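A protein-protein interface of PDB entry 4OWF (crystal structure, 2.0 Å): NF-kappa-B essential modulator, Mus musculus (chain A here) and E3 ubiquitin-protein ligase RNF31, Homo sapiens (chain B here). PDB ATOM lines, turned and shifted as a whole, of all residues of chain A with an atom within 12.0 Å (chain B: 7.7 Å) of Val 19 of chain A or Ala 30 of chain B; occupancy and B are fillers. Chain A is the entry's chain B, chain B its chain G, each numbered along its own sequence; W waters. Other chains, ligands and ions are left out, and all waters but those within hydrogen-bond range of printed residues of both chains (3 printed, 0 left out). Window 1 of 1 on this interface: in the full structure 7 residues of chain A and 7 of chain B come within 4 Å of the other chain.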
ATOM      1  N   GLN A  10      14.483   6.557  10.229  1.00  0.00           N
ATOM      2  CA  GLN A  10      15.621   5.646  10.149  1.00  0.00           C
ATOM      3  C   GLN A  10      16.945   6.417  10.200  1.00  0.00           C
ATOM      4  O   GLN A  10      17.900   5.989  10.850  1.00  0.00           O
ATOM      5  CB  GLN A  10      15.613   4.796   8.881  1.00  0.00           C
ATOM      6  CG  GLN A  10      14.610   3.680   8.827  1.00  0.00           C
ATOM      7  CD  GLN A  10      14.614   2.981   7.475  1.00  0.00           C
ATOM      8  OE1 GLN A  10      14.783   1.771   7.392  1.00  0.00           O
ATOM      9  NE2 GLN A  10      14.473   3.750   6.406  1.00  0.00           N
ATOM     10  N   LEU A  11      16.981   7.563   9.527  1.00  0.00           N
ATOM     11  CA  LEU A  11      18.182   8.342   9.419  1.00  0.00           C
ATOM     12  C   LEU A  11      18.565   8.887  10.784  1.00  0.00           C
ATOM     13  O   LEU A  11      19.708   8.777  11.191  1.00  0.00           O
ATOM     14  CB  LEU A  11      18.013   9.451   8.395  1.00  0.00           C
ATOM     15  CG  LEU A  11      19.187  10.401   8.190  1.00  0.00           C
ATOM     16  CD1 LEU A  11      20.380   9.647   7.650  1.00  0.00           C
ATOM     17  CD2 LEU A  11      18.813  11.531   7.249  1.00  0.00           C
ATOM     18  N   GLN A  12      17.584   9.415  11.505  1.00  0.00           N
ATOM     19  CA  GLN A  12      17.780   9.924  12.855  1.00  0.00           C
ATOM     20  C   GLN A  12      18.260   8.801  13.777  1.00  0.00           C
ATOM     21  O   GLN A  12      19.127   9.009  14.676  1.00  0.00           O
ATOM     22  CB  GLN A  12      16.468  10.512  13.363  1.00  0.00           C
ATOM     23  CG  GLN A  12      16.513  11.127  14.747  1.00  0.00           C
ATOM     24  CD  GLN A  12      17.506  12.284  14.874  1.00  0.00           C
ATOM     25  OE1 GLN A  12      17.978  12.586  15.969  1.00  0.00           O
ATOM     26  NE2 GLN A  12      17.814  12.935  13.772  1.00  0.00           N
ATOM     27  N   GLN A  13      17.719   7.603  13.564  1.00  0.00           N
ATOM     28  CA  GLN A  13      18.124   6.484  14.407  1.00  0.00           C
ATOM     29  C   GLN A  13      19.568   6.166  14.146  1.00  0.00           C
ATOM     30  O   GLN A  13      20.295   5.964  15.091  1.00  0.00           O
ATOM     31  CB  GLN A  13      17.300   5.244  14.170  1.00  0.00           C
ATOM     32  CG  GLN A  13      15.922   5.346  14.799  1.00  0.00           C
ATOM     33  CD  GLN A  13      15.151   4.076  14.581  1.00  0.00           C
ATOM     34  OE1 GLN A  13      14.768   3.776  13.471  1.00  0.00           O
ATOM     35  NE2 GLN A  13      15.008   3.286  15.620  1.00  0.00           N
ATOM     36  N   ALA A  14      19.936   6.052  12.871  1.00  0.00           N
ATOM     37  CA  ALA A  14      21.340   5.842  12.459  1.00  0.00           C
ATOM     38  C   ALA A  14      22.281   6.916  12.986  1.00  0.00           C
ATOM     39  O   ALA A  14      23.375   6.611  13.466  1.00  0.00           O
ATOM     40  CB  ALA A  14      21.433   5.783  10.952  1.00  0.00           C
ATOM     41  N   GLU A  15      21.851   8.185  12.891  1.00  0.00           N
ATOM     42  CA  GLU A  15      22.672   9.295  13.275  1.00  0.00           C
ATOM     43  C   GLU A  15      22.920   9.317  14.777  1.00  0.00           C
ATOM     44  O   GLU A  15      24.053   9.609  15.230  1.00  0.00           O
ATOM     45  CB  GLU A  15      22.103  10.599  12.729  1.00  0.00           C
ATOM     46  CG  GLU A  15      22.272  10.696  11.208  1.00  0.00           C
ATOM     47  CD  GLU A  15      22.187  12.143  10.673  1.00  0.00           C
ATOM     48  OE1 GLU A  15      21.049  12.679  10.502  1.00  0.00           O
ATOM     49  OE2 GLU A  15      23.261  12.746  10.385  1.00  0.00           O
ATOM     50  N   GLU A  16      21.906   8.950  15.552  1.00  0.00           N
ATOM     51  CA  GLU A  16      22.037   8.820  17.010  1.00  0.00           C
ATOM     52  C   GLU A  16      22.893   7.623  17.400  1.00  0.00           C
ATOM     53  O   GLU A  16      23.663   7.696  18.358  1.00  0.00           O
ATOM     54  CB  GLU A  16      20.651   8.652  17.658  1.00  0.00           C
ATOM     55  CG  GLU A  16      19.796   9.919  17.705  1.00  0.00           C
ATOM     56  CD  GLU A  16      18.319   9.637  18.041  1.00  0.00           C
ATOM     57  OE1 GLU A  16      17.880   8.461  18.015  1.00  0.00           O
ATOM     58  OE2 GLU A  16      17.577  10.601  18.297  1.00  0.00           O
ATOM     59  N   ALA A  17      22.734   6.506  16.698  1.00  0.00           N
ATOM     60  CA  ALA A  17      23.600   5.349  16.914  1.00  0.00           C
ATOM     61  C   ALA A  17      25.087   5.711  16.603  1.00  0.00           C
ATOM     62  O   ALA A  17      26.008   5.177  17.212  1.00  0.00           O
ATOM     63  CB  ALA A  17      23.158   4.183  16.031  1.00  0.00           C
ATOM     64  N   LEU A  18      25.331   6.551  15.609  1.00  0.00           N
ATOM     65  CA  LEU A  18      26.711   6.944  15.317  1.00  0.00           C
ATOM     66  C   LEU A  18      27.331   7.744  16.488  1.00  0.00           C
ATOM     67  O   LEU A  18      28.502   7.599  16.778  1.00  0.00           O
ATOM     68  CB  LEU A  18      26.798   7.728  14.026  1.00  0.00           C
ATOM     69  CG  LEU A  18      26.593   6.895  12.814  1.00  0.00           C
ATOM     70  CD1 LEU A  18      26.199   7.790  11.660  1.00  0.00           C
ATOM     71  CD2 LEU A  18      27.866   6.152  12.479  1.00  0.00           C
ATOM     72  N   VAL A  19      26.507   8.488  17.205  1.00  0.00           N
ATOM     73  CA  VAL A  19      26.963   9.182  18.398  1.00  0.00           C
ATOM     74  C   VAL A  19      27.380   8.158  19.470  1.00  0.00           C
ATOM     75  O   VAL A  19      28.404   8.366  20.119  1.00  0.00           O
ATOM     76  CB  VAL A  19      25.907  10.138  18.951  1.00  0.00           C
ATOM     77  CG1 VAL A  19      26.404  10.829  20.231  1.00  0.00           C
ATOM     78  CG2 VAL A  19      25.559  11.221  17.922  1.00  0.00           C
ATOM     79  N   ALA A  20      26.579   7.099  19.664  1.00  0.00           N
ATOM     80  CA  ALA A  20      26.863   6.087  20.682  1.00  0.00           C
ATOM     81  C   ALA A  20      28.123   5.334  20.292  1.00  0.00           C
ATOM     82  O   ALA A  20      28.922   5.030  21.128  1.00  0.00           O
ATOM     83  CB  ALA A  20      25.687   5.134  20.862  1.00  0.00           C
ATOM     84  N   LYS A  21      28.297   5.064  19.012  1.00  0.00           N
ATOM     85  CA  LYS A  21      29.529   4.499  18.536  1.00  0.00           C
ATOM     86  C   LYS A  21      30.730   5.441  18.786  1.00  0.00           C
ATOM     87  O   LYS A  21      31.760   4.987  19.323  1.00  0.00           O
ATOM     88  CB  LYS A  21      29.395   4.011  17.096  1.00  0.00           C
ATOM     89  CG  LYS A  21      28.695   2.642  17.066  1.00  0.00           C
ATOM     90  CD  LYS A  21      28.401   2.189  15.664  1.00  0.00           C
ATOM     91  CE  LYS A  21      28.380   0.674  15.513  1.00  0.00           C
ATOM     92  NZ  LYS A  21      27.496  -0.157  16.401  1.00  0.00           N
ATOM     93  N   GLN A  22      30.599   6.736  18.468  1.00  0.00           N
ATOM     94  CA  GLN A  22      31.706   7.634  18.698  1.00  0.00           C
ATOM     95  C   GLN A  22      32.097   7.729  20.167  1.00  0.00           C
ATOM     96  O   GLN A  22      33.268   7.822  20.456  1.00  0.00           O
ATOM     97  CB  GLN A  22      31.420   9.039  18.182  1.00  0.00           C
ATOM     98  CG  GLN A  22      32.681   9.885  18.109  1.00  0.00           C
ATOM     99  CD  GLN A  22      33.638   9.357  17.071  1.00  0.00           C
ATOM    100  OE1 GLN A  22      33.231   8.990  15.955  1.00  0.00           O
ATOM    101  NE2 GLN A  22      34.926   9.322  17.412  1.00  0.00           N
ATOM    102  N   GLU A  23      31.098   7.712  21.048  1.00  0.00           N
ATOM    103  CA  GLU A  23      31.270   7.723  22.512  1.00  0.00           C
ATOM    104  C   GLU A  23      32.121   6.546  23.049  1.00  0.00           C
ATOM    105  O   GLU A  23      32.930   6.689  23.992  1.00  0.00           O
ATOM    106  CB  GLU A  23      29.889   7.705  23.185  1.00  0.00           C
ATOM    107  CG  GLU A  23      29.309   9.087  23.470  1.00  0.00           C
ATOM    108  CD  GLU A  23      27.810   9.088  23.783  1.00  0.00           C
ATOM    109  OE1 GLU A  23      27.264  10.189  23.992  1.00  0.00           O
ATOM    110  OE2 GLU A  23      27.158   8.008  23.797  1.00  0.00           O
ATOM    111  N   LEU A  24      31.910   5.370  22.472  1.00  0.00           N
ATOM    112  CA  LEU A  24      32.695   4.196  22.861  1.00  0.00           C
ATOM    113  C   LEU A  24      34.107   4.331  22.274  1.00  0.00           C
ATOM    114  O   LEU A  24      35.096   4.115  22.963  1.00  0.00           O
ATOM    115  CB  LEU A  24      31.984   2.913  22.426  1.00  0.00           C
ATOM    116  CG  LEU A  24      32.708   1.578  22.622  1.00  0.00           C
ATOM    117  CD1 LEU A  24      33.156   1.457  24.082  1.00  0.00           C
ATOM    118  CD2 LEU A  24      31.781   0.418  22.207  1.00  0.00           C
ATOM    119  N   ILE A  25      34.216   4.761  21.024  1.00  0.00           N
ATOM    120  CA  ILE A  25      35.514   4.993  20.425  1.00  0.00           C
ATOM    121  C   ILE A  25      36.342   5.956  21.304  1.00  0.00           C
ATOM    122  O   ILE A  25      37.510   5.685  21.600  1.00  0.00           O
ATOM    123  CB  ILE A  25      35.345   5.586  19.001  1.00  0.00           C
ATOM    124  CG1 ILE A  25      34.863   4.489  18.056  1.00  0.00           C
ATOM    125  CG2 ILE A  25      36.652   6.154  18.460  1.00  0.00           C
ATOM    126  CD1 ILE A  25      34.589   4.972  16.641  1.00  0.00           C
ATOM    127  N   ASP A  26      35.710   7.053  21.733  1.00  0.00           N
ATOM    128  CA  ASP A  26      36.368   8.090  22.482  1.00  0.00           C
ATOM    129  C   ASP A  26      36.874   7.580  23.817  1.00  0.00           C
ATOM    130  O   ASP A  26      37.997   7.928  24.241  1.00  0.00           O
ATOM    131  CB  ASP A  26      35.449   9.295  22.678  1.00  0.00           C
ATOM    132  CG  ASP A  26      35.180  10.042  21.368  1.00  0.00           C
ATOM    133  OD1 ASP A  26      35.884   9.791  20.378  1.00  0.00           O
ATOM    134  OD2 ASP A  26      34.228  10.851  21.306  1.00  0.00           O
ATOM    135  N   LYS A  27      36.058   6.750  24.467  1.00  0.00           N
ATOM    136  CA  LYS A  27      36.454   6.118  25.732  1.00  0.00           C
ATOM    137  C   LYS A  27      37.607   5.106  25.542  1.00  0.00           C
ATOM    138  O   LYS A  27      38.544   5.058  26.351  1.00  0.00           O
ATOM    139  CB  LYS A  27      35.248   5.480  26.406  1.00  0.00           C
ATOM    140  CG  LYS A  27      35.543   4.390  27.434  1.00  0.00           C
ATOM    141  CD  LYS A  27      34.274   4.077  28.218  1.00  0.00           C
ATOM    142  CE  LYS A  27      34.409   2.833  29.076  1.00  0.00           C
ATOM    143  NZ  LYS A  27      34.655   1.635  28.239  1.00  0.00           N
ATOM    144  N   LEU A  28      37.543   4.310  24.484  1.00  0.00           N
ATOM    145  CA  LEU A  28      38.623   3.391  24.118  1.00  0.00           C
ATOM    146  C   LEU A  28      39.939   4.078  23.777  1.00  0.00           C
ATOM    147  O   LEU A  28      41.013   3.607  24.153  1.00  0.00           O
ATOM    148  CB  LEU A  28      38.200   2.469  22.966  1.00  0.00           C
ATOM    149  CG  LEU A  28      37.188   1.387  23.349  1.00  0.00           C
ATOM    150  CD1 LEU A  28      36.482   0.817  22.122  1.00  0.00           C
ATOM    151  CD2 LEU A  28      37.842   0.276  24.149  1.00  0.00           C
ATOM    152  N   LYS A  29      39.864   5.200  23.072  1.00  0.00           N
ATOM    153  CA  LYS A  29      41.064   5.954  22.748  1.00  0.00           C
ATOM    154  C   LYS A  29      41.713   6.551  23.991  1.00  0.00           C
ATOM    155  O   LYS A  29      42.932   6.643  24.068  1.00  0.00           O
ATOM    156  CB  LYS A  29      40.767   7.049  21.738  1.00  0.00           C
ATOM    157  CG  LYS A  29      40.778   6.554  20.306  1.00  0.00           C
ATOM    158  CD  LYS A  29      40.003   7.497  19.386  1.00  0.00           C
ATOM    159  CE  LYS A  29      40.581   8.910  19.339  1.00  0.00           C
ATOM    160  NZ  LYS A  29      41.574   9.100  18.247  1.00  0.00           N
ATOM    161  N   TRP B   5      26.507  22.191   7.919  1.00  0.00           N
ATOM    162  CA  TRP B   5      26.722  22.180   9.358  1.00  0.00           C
ATOM    163  C   TRP B   5      28.204  22.240   9.690  1.00  0.00           C
ATOM    164  O   TRP B   5      29.011  21.668   8.974  1.00  0.00           O
ATOM    165  CB  TRP B   5      26.052  20.960   9.985  1.00  0.00           C
ATOM    166  CG  TRP B   5      26.470  19.625   9.486  1.00  0.00           C
ATOM    167  CD1 TRP B   5      25.921  18.935   8.456  1.00  0.00           C
ATOM    168  CD2 TRP B   5      27.534  18.804   9.997  1.00  0.00           C
ATOM    169  NE1 TRP B   5      26.548  17.726   8.308  1.00  0.00           N
ATOM    170  CE2 TRP B   5      27.558  17.636   9.235  1.00  0.00           C
ATOM    171  CE3 TRP B   5      28.429  18.930  11.044  1.00  0.00           C
ATOM    172  CZ2 TRP B   5      28.447  16.612   9.486  1.00  0.00           C
ATOM    173  CZ3 TRP B   5      29.317  17.892  11.281  1.00  0.00           C
ATOM    174  CH2 TRP B   5      29.323  16.775  10.515  1.00  0.00           C
ATOM    175  N   CYS B   7      31.208  21.313  12.016  1.00  0.00           N
ATOM    176  CA  CYS B   7      31.586  20.283  12.978  1.00  0.00           C
ATOM    177  C   CYS B   7      31.978  20.935  14.297  1.00  0.00           C
ATOM    178  O   CYS B   7      32.816  21.848  14.311  1.00  0.00           O
ATOM    179  CB  CYS B   7      32.763  19.480  12.431  1.00  0.00           C
ATOM    180  SG  CYS B   7      33.491  18.237  13.521  1.00  0.00           S
ATOM    181  N   GLN B   8      31.436  20.430  15.407  1.00  0.00           N
ATOM    182  CA  GLN B   8      31.670  21.049  16.722  1.00  0.00           C
ATOM    183  C   GLN B   8      33.025  20.710  17.316  1.00  0.00           C
ATOM    184  O   GLN B   8      33.400  21.266  18.334  1.00  0.00           O
ATOM    185  CB  GLN B   8      30.541  20.685  17.718  1.00  0.00           C
ATOM    186  CG  GLN B   8      29.240  21.372  17.373  1.00  0.00           C
ATOM    187  CD  GLN B   8      29.439  22.887  17.200  1.00  0.00           C
ATOM    188  OE1 GLN B   8      29.690  23.619  18.174  1.00  0.00           O
ATOM    189  NE2 GLN B   8      29.385  23.354  15.951  1.00  0.00           N
ATOM    190  N   SER B   9      33.765  19.830  16.672  1.00  0.00           N
ATOM    191  CA  SER B   9      35.072  19.408  17.157  1.00  0.00           C
ATOM    192  C   SER B   9      36.242  20.061  16.375  1.00  0.00           C
ATOM    193  O   SER B   9      37.209  20.500  16.971  1.00  0.00           O
ATOM    194  CB  SER B   9      35.175  17.891  17.104  1.00  0.00           C
ATOM    195  OG  SER B   9      36.521  17.502  17.293  1.00  0.00           O
ATOM    196  N   VAL B  19      26.956  12.772   6.874  1.00  0.00           N
ATOM    197  CA  VAL B  19      26.671  12.058   8.071  1.00  0.00           C
ATOM    198  C   VAL B  19      27.856  12.116   9.074  1.00  0.00           C
ATOM    199  O   VAL B  19      27.670  12.169  10.296  1.00  0.00           O
ATOM    200  CB  VAL B  19      26.294  10.627   7.576  1.00  0.00           C
ATOM    201  CG1 VAL B  19      26.297   9.587   8.653  1.00  0.00           C
ATOM    202  CG2 VAL B  19      24.930  10.689   6.923  1.00  0.00           C
ATOM    203  N   LEU B  20      29.077  12.070   8.546  1.00  0.00           N
ATOM    204  CA  LEU B  20      30.295  12.242   9.336  1.00  0.00           C
ATOM    205  C   LEU B  20      31.029  13.517   8.877  1.00  0.00           C
ATOM    206  O   LEU B  20      30.921  13.904   7.714  1.00  0.00           O
ATOM    207  CB  LEU B  20      31.227  11.062   9.102  1.00  0.00           C
ATOM    208  CG  LEU B  20      30.686   9.652   9.372  1.00  0.00           C
ATOM    209  CD1 LEU B  20      31.776   8.652   9.051  1.00  0.00           C
ATOM    210  CD2 LEU B  20      30.198   9.475  10.798  1.00  0.00           C
ATOM    211  N   ARG B  26      34.017  12.664  12.710  1.00  0.00           N
ATOM    212  CA  ARG B  26      33.053  12.594  13.789  1.00  0.00           C
ATOM    213  C   ARG B  26      31.600  12.760  13.301  1.00  0.00           C
ATOM    214  O   ARG B  26      31.337  13.519  12.373  1.00  0.00           O
ATOM    215  CB  ARG B  26      33.356  13.647  14.858  1.00  0.00           C
ATOM    216  CG  ARG B  26      34.625  13.293  15.620  1.00  0.00           C
ATOM    217  CD  ARG B  26      34.906  14.224  16.783  1.00  0.00           C
ATOM    218  NE  ARG B  26      34.456  13.608  18.026  1.00  0.00           N
ATOM    219  CZ  ARG B  26      33.317  13.880  18.630  1.00  0.00           C
ATOM    220  NH1 ARG B  26      32.486  14.779  18.118  1.00  0.00           N
ATOM    221  NH2 ARG B  26      33.008  13.244  19.750  1.00  0.00           N
ATOM    222  N   PRO B  27      30.666  12.016  13.910  1.00  0.00           N
ATOM    223  CA  PRO B  27      29.247  12.121  13.473  1.00  0.00           C
ATOM    224  C   PRO B  27      28.693  13.523  13.665  1.00  0.00           C
ATOM    225  O   PRO B  27      29.118  14.236  14.579  1.00  0.00           O
ATOM    226  CB  PRO B  27      28.505  11.161  14.398  1.00  0.00           C
ATOM    227  CG  PRO B  27      29.517  10.348  15.080  1.00  0.00           C
ATOM    228  CD  PRO B  27      30.890  10.930  14.875  1.00  0.00           C
ATOM    229  N   ARG B  28      27.723  13.896  12.847  1.00  0.00           N
ATOM    230  CA  ARG B  28      27.066  15.233  12.913  1.00  0.00           C
ATOM    231  C   ARG B  28      26.548  15.640  14.298  1.00  0.00           C
ATOM    232  O   ARG B  28      26.653  16.806  14.696  1.00  0.00           O
ATOM    233  CB  ARG B  28      25.935  15.253  11.874  1.00  0.00           C
ATOM    234  CG  ARG B  28      25.207  16.577  11.700  1.00  0.00           C
ATOM    235  CD  ARG B  28      24.192  16.468  10.556  1.00  0.00           C
ATOM    236  NE  ARG B  28      23.054  15.620  10.884  1.00  0.00           N
ATOM    237  CZ  ARG B  28      22.029  16.004  11.649  1.00  0.00           C
ATOM    238  NH1 ARG B  28      21.033  15.174  11.905  1.00  0.00           N
ATOM    239  NH2 ARG B  28      21.996  17.215  12.187  1.00  0.00           N
ATOM    240  N   LEU B  29      25.969  14.696  15.042  1.00  0.00           N
ATOM    241  CA  LEU B  29      25.319  15.013  16.315  1.00  0.00           C
ATOM    242  C   LEU B  29      26.178  14.749  17.549  1.00  0.00           C
ATOM    243  O   LEU B  29      25.677  14.872  18.655  1.00  0.00           O
ATOM    244  CB  LEU B  29      24.035  14.216  16.465  1.00  0.00           C
ATOM    245  CG  LEU B  29      22.986  14.433  15.390  1.00  0.00           C
ATOM    246  CD1 LEU B  29      21.788  13.520  15.649  1.00  0.00           C
ATOM    247  CD2 LEU B  29      22.552  15.903  15.341  1.00  0.00           C
ATOM    248  N   ALA B  30      27.445  14.382  17.371  1.00  0.00           N
ATOM    249  CA  ALA B  30      28.295  13.983  18.490  1.00  0.00           C
ATOM    250  C   ALA B  30      28.760  15.203  19.266  1.00  0.00           C
ATOM    251  O   ALA B  30      29.265  16.147  18.658  1.00  0.00           O
ATOM    252  CB  ALA B  30      29.498  13.209  17.997  1.00  0.00           C
HETATM  253  O   HOH W   1      35.823  10.502  14.520  1.00  0.00           O
HETATM  254  O   HOH W   2      25.330  11.510  11.289  1.00  0.00           O
HETATM  255  O   HOH W   3      25.354  11.783  14.024  1.00  0.00           O
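OE1 of Glu 15 of chain A is in salt-bridge range of NH1 of Arg 28 of chain B (2.9 Å).
OD2 of Asp 26 of chain A lies within salt-bridge range of NH2 of Arg 26 of chain B (3.1 Å).
The side-chain amide oxygen (OE1) of Gln 12 of chain A sits close to the side-chain carboxylate (OE2) of Glu 16 of chain A (3.1 Å).
The side-chain amide nitrogen of Gln 22 of chain A is in hydrogen-bond range of the side-chain carboxylate of Asp 26 of chain A, 3.2 Å away.
N of Arg 28 of chain B sits at hydrogen-bond distance from O of Val 19 of chain B, at 3.1 Å.
Leu 29 of chain B touches Gln 12 of chain A.
Val 19 of chain B touches Leu 18 of chain A.
CG of Pro 27 of chain B touches O of Leu 18 of chain A (3.4 Å).
Val 19 of chain A touches Leu 29 of chain B.
N of Ala 30 of chain B touches CG2 of Val 19 of chain A (3.7 Å).
Arg 26 of chain B touches Gln 22 of chain A (NH2 to CG, 3.8 Å).
Gln 22 of chain A touches Pro 27 of chain B.
Of chain B, only Leu 29 and Ala 30 come within 4 Å of Val 19 of chain A.
Ala 30 of chain B touches one residue of chain A.
Arg 26 of chain B touches just these residues of chain A: Gln 22 and Asp 26.
Pro 27 of chain B touches just these residues of chain A: Leu 18 (3.4 Å) and Gln 22 (3.2 Å).
Leu 29 of chain B touches just these residues of chain A: Gln 12 and Val 19.
Printed residues of chain B within 4 Å of Leu 18 of chain A: Val 19 (3.5 Å) and Pro 27 (3.4 Å).
Printed residues of chain B within 4 Å of Gln 12 of chain A: Leu 29.
Printed residues of chain B within 4 Å of Asp 26 of chain A: Arg 26 (3.1 Å).
Ala 17 of chain A touches none of the printed residues of chain B.
Gln 13 of chain A touches none of the printed residues of chain B.
The nearest residue of chain B that does not touch Val 19 of chain A is Pro 27 of chain B (4.1 Å).
The nearest residue of chain A that does not touch Ala 30 of chain B is Gln 22 of chain A (4.6 Å).
Of the 11 printed residues of chain B, 6 touch a printed residue of chain A.
Hydrophobic or aromatic side chains of chain B that line the printed part of chain A: Val 19, Pro 27 and Leu 29.
Printed residues of chain A that touch a printed residue of chain B: Gln 12, Glu 15, Leu 18, Val 19, Gln 22 and Asp 26.
Hydrophobic or aromatic side chains of chain A within 4 Å of the printed part of chain B: Leu 18 and Val 19.
Along chain A the printed residues that touch a printed residue of chain B span positions 12 to 26.
Among the printed residues, Asp or Glu carboxylates within 4 Å of a Lys or Arg side-chain nitrogen of the other chain: Glu 15 of chain A with Arg 28 of chain B (2.9 Å) and Asp 26 of chain A with Arg 26 of chain B (3.1 Å).
Water W2 lies within hydrogen-bond range of the side-chain carboxylate of Glu 15 of chain A (2.6 Å) and the backbone carbonyl oxygen of Val 19 of chain B (2.6 Å).
Water W3 lies within hydrogen-bond range of O of Glu 15 of chain A (2.8 Å), N of Leu 29 of chain B (3.1 Å) and N of Arg 28 of chain B (3.4 Å).
Water W1 lies within hydrogen-bond range of NE2 of Gln 22 of chain A (3.2 Å) and N of Arg 26 of chain B (3.3 Å).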
